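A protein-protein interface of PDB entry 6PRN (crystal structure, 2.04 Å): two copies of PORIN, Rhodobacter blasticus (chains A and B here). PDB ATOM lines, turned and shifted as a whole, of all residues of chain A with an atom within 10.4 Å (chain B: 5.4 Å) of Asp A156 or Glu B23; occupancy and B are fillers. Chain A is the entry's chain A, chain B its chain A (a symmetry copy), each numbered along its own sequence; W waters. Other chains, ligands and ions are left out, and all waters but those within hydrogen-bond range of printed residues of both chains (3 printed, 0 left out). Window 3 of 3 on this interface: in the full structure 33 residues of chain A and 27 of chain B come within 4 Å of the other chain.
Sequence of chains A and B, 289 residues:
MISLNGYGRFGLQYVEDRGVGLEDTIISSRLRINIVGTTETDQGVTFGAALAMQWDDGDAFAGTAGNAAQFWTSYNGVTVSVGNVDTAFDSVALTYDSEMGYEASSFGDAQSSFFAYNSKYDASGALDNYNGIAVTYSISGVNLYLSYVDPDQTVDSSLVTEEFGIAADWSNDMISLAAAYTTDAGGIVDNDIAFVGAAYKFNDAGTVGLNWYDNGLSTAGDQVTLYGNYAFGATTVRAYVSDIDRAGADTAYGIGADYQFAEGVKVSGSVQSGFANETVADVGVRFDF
N of Glu B23 is in hydrogen-bond range of O of Thr A154 (2.8 Å).
N of Asp A156 is in hydrogen-bond range of O of Gly B21 (3.0 Å).
The side-chain hydroxyl of Ser A157 lies within hydrogen-bond range of the side-chain carboxylate of Glu B23.
O of Asn A129 sits at hydrogen-bond distance from N of Gln A153 (2.9 Å).
OD1 of Asp A152 sits at hydrogen-bond distance from OG1 of Thr A154, 2.8 Å away.
The backbone NH (N) of Ser A158 lies within hydrogen-bond range of the side-chain carboxylate (OD1) of Asp A156 (3.0 Å).
The guanidinium group of Arg B18 sits at hydrogen-bond distance from the backbone carbonyl oxygen of Glu B23.
O of Gln A153 touches CB of Glu B23, 3.8 Å away.
Gln A153 touches Ile B26.
O of Thr A154 touches CA of Leu B22, at 3.4 Å.
Gly B21 touches Val A155.
Glu B23 touches Val A155.
CA of Asp A156 touches OE2 of Glu B23, 3.4 Å away.
Of the printed residues of chain B, Gln A153 touches Glu B23 (3.8 Å) and Ile B26 (3.7 Å).
Of the printed residues of chain B, Val A155 touches Gly B21 (3.7 Å) and Glu B23 (3.97 Å).
Of the printed residues of chain B, Asp A156 touches Gly B21 (3.0 Å) and Glu B23 (3.4 Å).
Of the printed residues of chain B, Ser A157 touches Glu B23 (2.8 Å).
Printed residues of chain A within 4 Å of Ile B26: Gln A153.
The nearest residue of chain B that does not touch Asp A156 is Leu B22 (4.2 Å).
Printed residues of chain B that touch a printed residue of chain A: Gly B21, Leu B22, Glu B23 and Ile B26.
Of the 15 printed residues of chain A, 5 touch a printed residue of chain B.
Printed residues of chain A that touch a printed residue of chain B: Gln A153, Thr A154, Val A155, Asp A156 and Ser A157.
Hydrophobic or aromatic side chains of chain A within 4 Å of the printed part of chain B: Val A155.
Among the printed residues, no Asp or Glu carboxylate lies within 4 Å of a Lys or Arg side-chain nitrogen of the other chain.
No position is printed for both chains.
Water W1 lies within hydrogen-bond range of O of Gln A153 (2.6 Å) and O of Thr B25 (3.1 Å).
Water W2 bridges the backbone carbonyl oxygen (O) of Thr A154 (2.7 Å) and the backbone carbonyl oxygen (O) of Glu B23 (2.9 Å).
Water W3 bridges O of Leu B22 and OD2 of Asp A156.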
ATOM      1  N   ASN A 129     -20.056   4.532  13.115  1.00  0.00           N
ATOM      2  CA  ASN A 129     -20.173   5.805  12.394  1.00  0.00           C
ATOM      3  C   ASN A 129     -21.055   5.649  11.168  1.00  0.00           C
ATOM      4  O   ASN A 129     -20.897   6.373  10.175  1.00  0.00           O
ATOM      5  CB  ASN A 129     -18.746   6.235  11.949  1.00  0.00           C
ATOM      6  CG  ASN A 129     -17.954   6.670  13.178  1.00  0.00           C
ATOM      7  OD1 ASN A 129     -18.304   7.673  13.804  1.00  0.00           O
ATOM      8  ND2 ASN A 129     -16.927   5.954  13.585  1.00  0.00           N
ATOM      9  N   TYR A 148     -29.604   6.433   0.880  1.00  0.00           N
ATOM     10  CA  TYR A 148     -28.164   6.521   0.739  1.00  0.00           C
ATOM     11  C   TYR A 148     -27.547   6.198   2.100  1.00  0.00           C
ATOM     12  O   TYR A 148     -27.940   6.806   3.116  1.00  0.00           O
ATOM     13  CB  TYR A 148     -27.794   7.961   0.327  1.00  0.00           C
ATOM     14  CG  TYR A 148     -26.313   8.235   0.479  1.00  0.00           C
ATOM     15  CD1 TYR A 148     -25.423   7.882  -0.528  1.00  0.00           C
ATOM     16  CD2 TYR A 148     -25.832   8.840   1.622  1.00  0.00           C
ATOM     17  CE1 TYR A 148     -24.064   8.171  -0.402  1.00  0.00           C
ATOM     18  CE2 TYR A 148     -24.484   9.122   1.778  1.00  0.00           C
ATOM     19  CZ  TYR A 148     -23.619   8.777   0.757  1.00  0.00           C
ATOM     20  OH  TYR A 148     -22.269   9.038   0.908  1.00  0.00           O
ATOM     21  N   ASP A 150     -24.008   5.556   4.248  1.00  0.00           N
ATOM     22  CA  ASP A 150     -22.532   5.572   4.336  1.00  0.00           C
ATOM     23  C   ASP A 150     -22.167   4.818   5.601  1.00  0.00           C
ATOM     24  O   ASP A 150     -22.465   5.299   6.712  1.00  0.00           O
ATOM     25  CB  ASP A 150     -22.118   7.024   4.391  1.00  0.00           C
ATOM     26  CG  ASP A 150     -20.608   7.231   4.416  1.00  0.00           C
ATOM     27  OD1 ASP A 150     -19.903   6.260   4.645  1.00  0.00           O
ATOM     28  OD2 ASP A 150     -20.169   8.384   4.192  1.00  0.00           O
ATOM     29  N   PRO A 151     -21.510   3.682   5.490  1.00  0.00           N
ATOM     30  CA  PRO A 151     -21.138   2.846   6.612  1.00  0.00           C
ATOM     31  C   PRO A 151     -20.144   3.431   7.573  1.00  0.00           C
ATOM     32  O   PRO A 151     -20.074   2.976   8.726  1.00  0.00           O
ATOM     33  CB  PRO A 151     -20.693   1.530   6.003  1.00  0.00           C
ATOM     34  CG  PRO A 151     -20.409   1.794   4.561  1.00  0.00           C
ATOM     35  CD  PRO A 151     -21.141   3.052   4.187  1.00  0.00           C
ATOM     36  N   ASP A 152     -19.383   4.443   7.194  1.00  0.00           N
ATOM     37  CA  ASP A 152     -18.470   5.119   8.077  1.00  0.00           C
ATOM     38  C   ASP A 152     -18.307   6.547   7.589  1.00  0.00           C
ATOM     39  O   ASP A 152     -17.373   6.856   6.799  1.00  0.00           O
ATOM     40  CB  ASP A 152     -17.110   4.427   8.192  1.00  0.00           C
ATOM     41  CG  ASP A 152     -16.261   5.029   9.291  1.00  0.00           C
ATOM     42  OD1 ASP A 152     -16.406   6.219   9.644  1.00  0.00           O
ATOM     43  OD2 ASP A 152     -15.338   4.317   9.740  1.00  0.00           O
ATOM     44  N   GLN A 153     -19.222   7.419   8.042  1.00  0.00           N
ATOM     45  CA  GLN A 153     -19.231   8.786   7.570  1.00  0.00           C
ATOM     46  C   GLN A 153     -18.067   9.636   7.988  1.00  0.00           C
ATOM     47  O   GLN A 153     -17.930  10.756   7.445  1.00  0.00           O
ATOM     48  CB  GLN A 153     -20.565   9.487   7.987  1.00  0.00           C
ATOM     49  CG  GLN A 153     -20.568   9.837   9.506  1.00  0.00           C
ATOM     50  CD  GLN A 153     -21.617  10.906   9.804  1.00  0.00           C
ATOM     51  OE1 GLN A 153     -22.016  11.706   8.946  1.00  0.00           O
ATOM     52  NE2 GLN A 153     -22.060  10.970  11.072  1.00  0.00           N
ATOM     53  N   THR A 154     -17.251   9.281   8.950  1.00  0.00           N
ATOM     54  CA  THR A 154     -16.164  10.152   9.356  1.00  0.00           C
ATOM     55  C   THR A 154     -14.963   9.998   8.381  1.00  0.00           C
ATOM     56  O   THR A 154     -14.123  10.889   8.368  1.00  0.00           O
ATOM     57  CB  THR A 154     -15.658   9.810  10.766  1.00  0.00           C
ATOM     58  OG1 THR A 154     -15.144   8.459  10.646  1.00  0.00           O
ATOM     59  CG2 THR A 154     -16.760   9.812  11.817  1.00  0.00           C
ATOM     60  N   VAL A 155     -14.859   8.910   7.662  1.00  0.00           N
ATOM     61  CA  VAL A 155     -13.676   8.688   6.776  1.00  0.00           C
ATOM     62  C   VAL A 155     -13.941   9.277   5.413  1.00  0.00           C
ATOM     63  O   VAL A 155     -15.082   9.363   4.938  1.00  0.00           O
ATOM     64  CB  VAL A 155     -13.422   7.169   6.679  1.00  0.00           C
ATOM     65  CG1 VAL A 155     -12.452   6.829   5.554  1.00  0.00           C
ATOM     66  CG2 VAL A 155     -12.899   6.645   8.012  1.00  0.00           C
ATOM     67  N   ASP A 156     -12.880   9.747   4.735  1.00  0.00           N
ATOM     68  CA  ASP A 156     -13.083  10.323   3.395  1.00  0.00           C
ATOM     69  C   ASP A 156     -13.988   9.431   2.555  1.00  0.00           C
ATOM     70  O   ASP A 156     -13.752   8.207   2.491  1.00  0.00           O
ATOM     71  CB  ASP A 156     -11.702  10.411   2.696  1.00  0.00           C
ATOM     72  CG  ASP A 156     -11.815  11.288   1.457  1.00  0.00           C
ATOM     73  OD1 ASP A 156     -12.336  10.807   0.380  1.00  0.00           O
ATOM     74  OD2 ASP A 156     -11.420  12.510   1.504  1.00  0.00           O
ATOM     75  N   SER A 157     -14.983   9.983   1.875  1.00  0.00           N
ATOM     76  CA  SER A 157     -15.918   9.216   1.077  1.00  0.00           C
ATOM     77  C   SER A 157     -15.336   8.298   0.024  1.00  0.00           C
ATOM     78  O   SER A 157     -15.932   7.265  -0.316  1.00  0.00           O
ATOM     79  CB  SER A 157     -16.902  10.153   0.314  1.00  0.00           C
ATOM     80  OG  SER A 157     -17.261  11.198   1.198  1.00  0.00           O
ATOM     81  N   SER A 158     -14.209   8.672  -0.590  1.00  0.00           N
ATOM     82  CA  SER A 158     -13.594   7.843  -1.626  1.00  0.00           C
ATOM     83  C   SER A 158     -12.964   6.583  -1.066  1.00  0.00           C
ATOM     84  O   SER A 158     -12.638   5.649  -1.839  1.00  0.00           O
ATOM     85  CB  SER A 158     -12.528   8.680  -2.369  1.00  0.00           C
ATOM     86  OG  SER A 158     -11.347   8.744  -1.563  1.00  0.00           O
ATOM     87  N   LEU A 159     -12.763   6.482   0.240  1.00  0.00           N
ATOM     88  CA  LEU A 159     -12.180   5.299   0.840  1.00  0.00           C
ATOM     89  C   LEU A 159     -13.192   4.270   1.315  1.00  0.00           C
ATOM     90  O   LEU A 159     -12.814   3.199   1.822  1.00  0.00           O
ATOM     91  CB  LEU A 159     -11.319   5.758   2.049  1.00  0.00           C
ATOM     92  CG  LEU A 159     -10.107   6.621   1.617  1.00  0.00           C
ATOM     93  CD1 LEU A 159      -9.569   7.438   2.776  1.00  0.00           C
ATOM     94  CD2 LEU A 159      -9.010   5.696   1.082  1.00  0.00           C
ATOM     95  N   VAL A 160     -14.486   4.597   1.267  1.00  0.00           N
ATOM     96  CA  VAL A 160     -15.533   3.712   1.767  1.00  0.00           C
ATOM     97  C   VAL A 160     -16.576   3.471   0.681  1.00  0.00           C
ATOM     98  O   VAL A 160     -16.807   4.330  -0.164  1.00  0.00           O
ATOM     99  CB  VAL A 160     -16.151   4.196   3.089  1.00  0.00           C
ATOM    100  CG1 VAL A 160     -15.628   5.531   3.583  1.00  0.00           C
ATOM    101  CG2 VAL A 160     -17.668   4.234   3.099  1.00  0.00           C
ATOM    102  N   THR A 161     -17.182   2.310   0.660  1.00  0.00           N
ATOM    103  CA  THR A 161     -18.236   2.018  -0.325  1.00  0.00           C
ATOM    104  C   THR A 161     -19.606   2.408   0.231  1.00  0.00           C
ATOM    105  O   THR A 161     -19.979   1.887   1.277  1.00  0.00           O
ATOM    106  CB  THR A 161     -18.264   0.503  -0.613  1.00  0.00           C
ATOM    107  OG1 THR A 161     -16.966   0.155  -1.114  1.00  0.00           O
ATOM    108  CG2 THR A 161     -19.348   0.131  -1.597  1.00  0.00           C
ATOM    109  N   GLU A 162     -20.318   3.279  -0.426  1.00  0.00           N
ATOM    110  CA  GLU A 162     -21.635   3.715   0.025  1.00  0.00           C
ATOM    111  C   GLU A 162     -22.715   2.970  -0.740  1.00  0.00           C
ATOM    112  O   GLU A 162     -22.475   2.582  -1.892  1.00  0.00           O
ATOM    113  CB  GLU A 162     -21.798   5.228  -0.149  1.00  0.00           C
ATOM    114  CG  GLU A 162     -20.867   5.992   0.798  1.00  0.00           C
ATOM    115  CD  GLU A 162     -19.625   6.472   0.059  1.00  0.00           C
ATOM    116  OE1 GLU A 162     -19.616   6.421  -1.189  1.00  0.00           O
ATOM    117  OE2 GLU A 162     -18.639   6.883   0.717  1.00  0.00           O
ATOM    118  N   ARG B  18     -10.002  18.414   9.837  1.00  0.00           N
ATOM    119  CA  ARG B  18     -10.259  17.513  10.945  1.00  0.00           C
ATOM    120  C   ARG B  18      -9.204  16.452  11.152  1.00  0.00           C
ATOM    121  O   ARG B  18      -8.900  16.098  12.306  1.00  0.00           O
ATOM    122  CB  ARG B  18     -11.633  16.858  10.690  1.00  0.00           C
ATOM    123  CG  ARG B  18     -12.270  16.251  11.905  1.00  0.00           C
ATOM    124  CD  ARG B  18     -13.507  15.480  11.469  1.00  0.00           C
ATOM    125  NE  ARG B  18     -14.665  16.303  11.209  1.00  0.00           N
ATOM    126  CZ  ARG B  18     -15.605  16.679  12.078  1.00  0.00           C
ATOM    127  NH1 ARG B  18     -15.528  16.354  13.378  1.00  0.00           N
ATOM    128  NH2 ARG B  18     -16.637  17.409  11.660  1.00  0.00           N
ATOM    129  N   GLY B  19      -8.635  15.897  10.081  1.00  0.00           N
ATOM    130  CA  GLY B  19      -7.618  14.846  10.261  1.00  0.00           C
ATOM    131  C   GLY B  19      -7.293  14.178   8.926  1.00  0.00           C
ATOM    132  O   GLY B  19      -8.068  14.209   7.966  1.00  0.00           O
ATOM    133  N   GLY B  21      -7.183  11.850   6.085  1.00  0.00           N
ATOM    134  CA  GLY B  21      -8.134  10.863   5.606  1.00  0.00           C
ATOM    135  C   GLY B  21      -9.507  10.952   6.299  1.00  0.00           C
ATOM    136  O   GLY B  21     -10.250   9.969   6.226  1.00  0.00           O
ATOM    137  N   LEU B  22      -9.814  12.061   6.956  1.00  0.00           N
ATOM    138  CA  LEU B  22     -11.123  12.205   7.607  1.00  0.00           C
ATOM    139  C   LEU B  22     -11.901  13.272   6.845  1.00  0.00           C
ATOM    140  O   LEU B  22     -11.340  14.214   6.292  1.00  0.00           O
ATOM    141  CB  LEU B  22     -11.053  12.579   9.070  1.00  0.00           C
ATOM    142  CG  LEU B  22     -10.374  11.639  10.054  1.00  0.00           C
ATOM    143  CD1 LEU B  22     -10.312  12.262  11.445  1.00  0.00           C
ATOM    144  CD2 LEU B  22     -11.004  10.268  10.110  1.00  0.00           C
ATOM    145  N   GLU B  23     -13.213  13.116   6.880  1.00  0.00           N
ATOM    146  CA  GLU B  23     -14.120  14.073   6.251  1.00  0.00           C
ATOM    147  C   GLU B  23     -14.211  15.290   7.173  1.00  0.00           C
ATOM    148  O   GLU B  23     -14.421  15.143   8.384  1.00  0.00           O
ATOM    149  CB  GLU B  23     -15.478  13.398   6.128  1.00  0.00           C
ATOM    150  CG  GLU B  23     -16.356  13.657   4.900  1.00  0.00           C
ATOM    151  CD  GLU B  23     -15.619  13.738   3.584  1.00  0.00           C
ATOM    152  OE1 GLU B  23     -15.160  14.880   3.229  1.00  0.00           O
ATOM    153  OE2 GLU B  23     -15.482  12.702   2.834  1.00  0.00           O
ATOM    154  N   ASP B  24     -14.125  16.497   6.633  1.00  0.00           N
ATOM    155  CA  ASP B  24     -14.229  17.673   7.487  1.00  0.00           C
ATOM    156  C   ASP B  24     -15.701  17.925   7.909  1.00  0.00           C
ATOM    157  O   ASP B  24     -15.919  18.417   9.009  1.00  0.00           O
ATOM    158  CB  ASP B  24     -13.793  18.916   6.693  1.00  0.00           C
ATOM    159  CG  ASP B  24     -12.267  19.091   6.665  1.00  0.00           C
ATOM    160  OD1 ASP B  24     -11.535  18.414   7.387  1.00  0.00           O
ATOM    161  OD2 ASP B  24     -11.873  19.985   5.898  1.00  0.00           O
ATOM    162  N   THR B  25     -16.620  17.587   7.015  1.00  0.00           N
ATOM    163  CA  THR B  25     -18.042  17.817   7.340  1.00  0.00           C
ATOM    164  C   THR B  25     -18.748  16.490   7.588  1.00  0.00           C
ATOM    165  O   THR B  25     -18.626  15.564   6.770  1.00  0.00           O
ATOM    166  CB  THR B  25     -18.736  18.569   6.206  1.00  0.00           C
ATOM    167  OG1 THR B  25     -18.147  19.872   6.027  1.00  0.00           O
ATOM    168  CG2 THR B  25     -20.239  18.808   6.533  1.00  0.00           C
ATOM    169  N   ILE B  26     -19.381  16.338   8.762  1.00  0.00           N
ATOM    170  CA  ILE B  26     -20.162  15.132   9.018  1.00  0.00           C
ATOM    171  C   ILE B  26     -21.615  15.537   9.446  1.00  0.00           C
ATOM    172  O   ILE B  26     -21.902  16.699   9.668  1.00  0.00           O
ATOM    173  CB  ILE B  26     -19.569  14.270  10.139  1.00  0.00           C
ATOM    174  CG1 ILE B  26     -19.602  15.031  11.474  1.00  0.00           C
ATOM    175  CG2 ILE B  26     -18.143  13.812   9.819  1.00  0.00           C
ATOM    176  CD1 ILE B  26     -19.230  14.163  12.660  1.00  0.00           C
HETATM  177  O   HOH W   1     -19.150  12.595   6.015  1.00  0.00           O
HETATM  178  O   HOH W   2     -14.574  12.872  10.121  1.00  0.00           O
HETATM  179  O   HOH W   3      -9.671  14.016   3.784  1.00  0.00           O
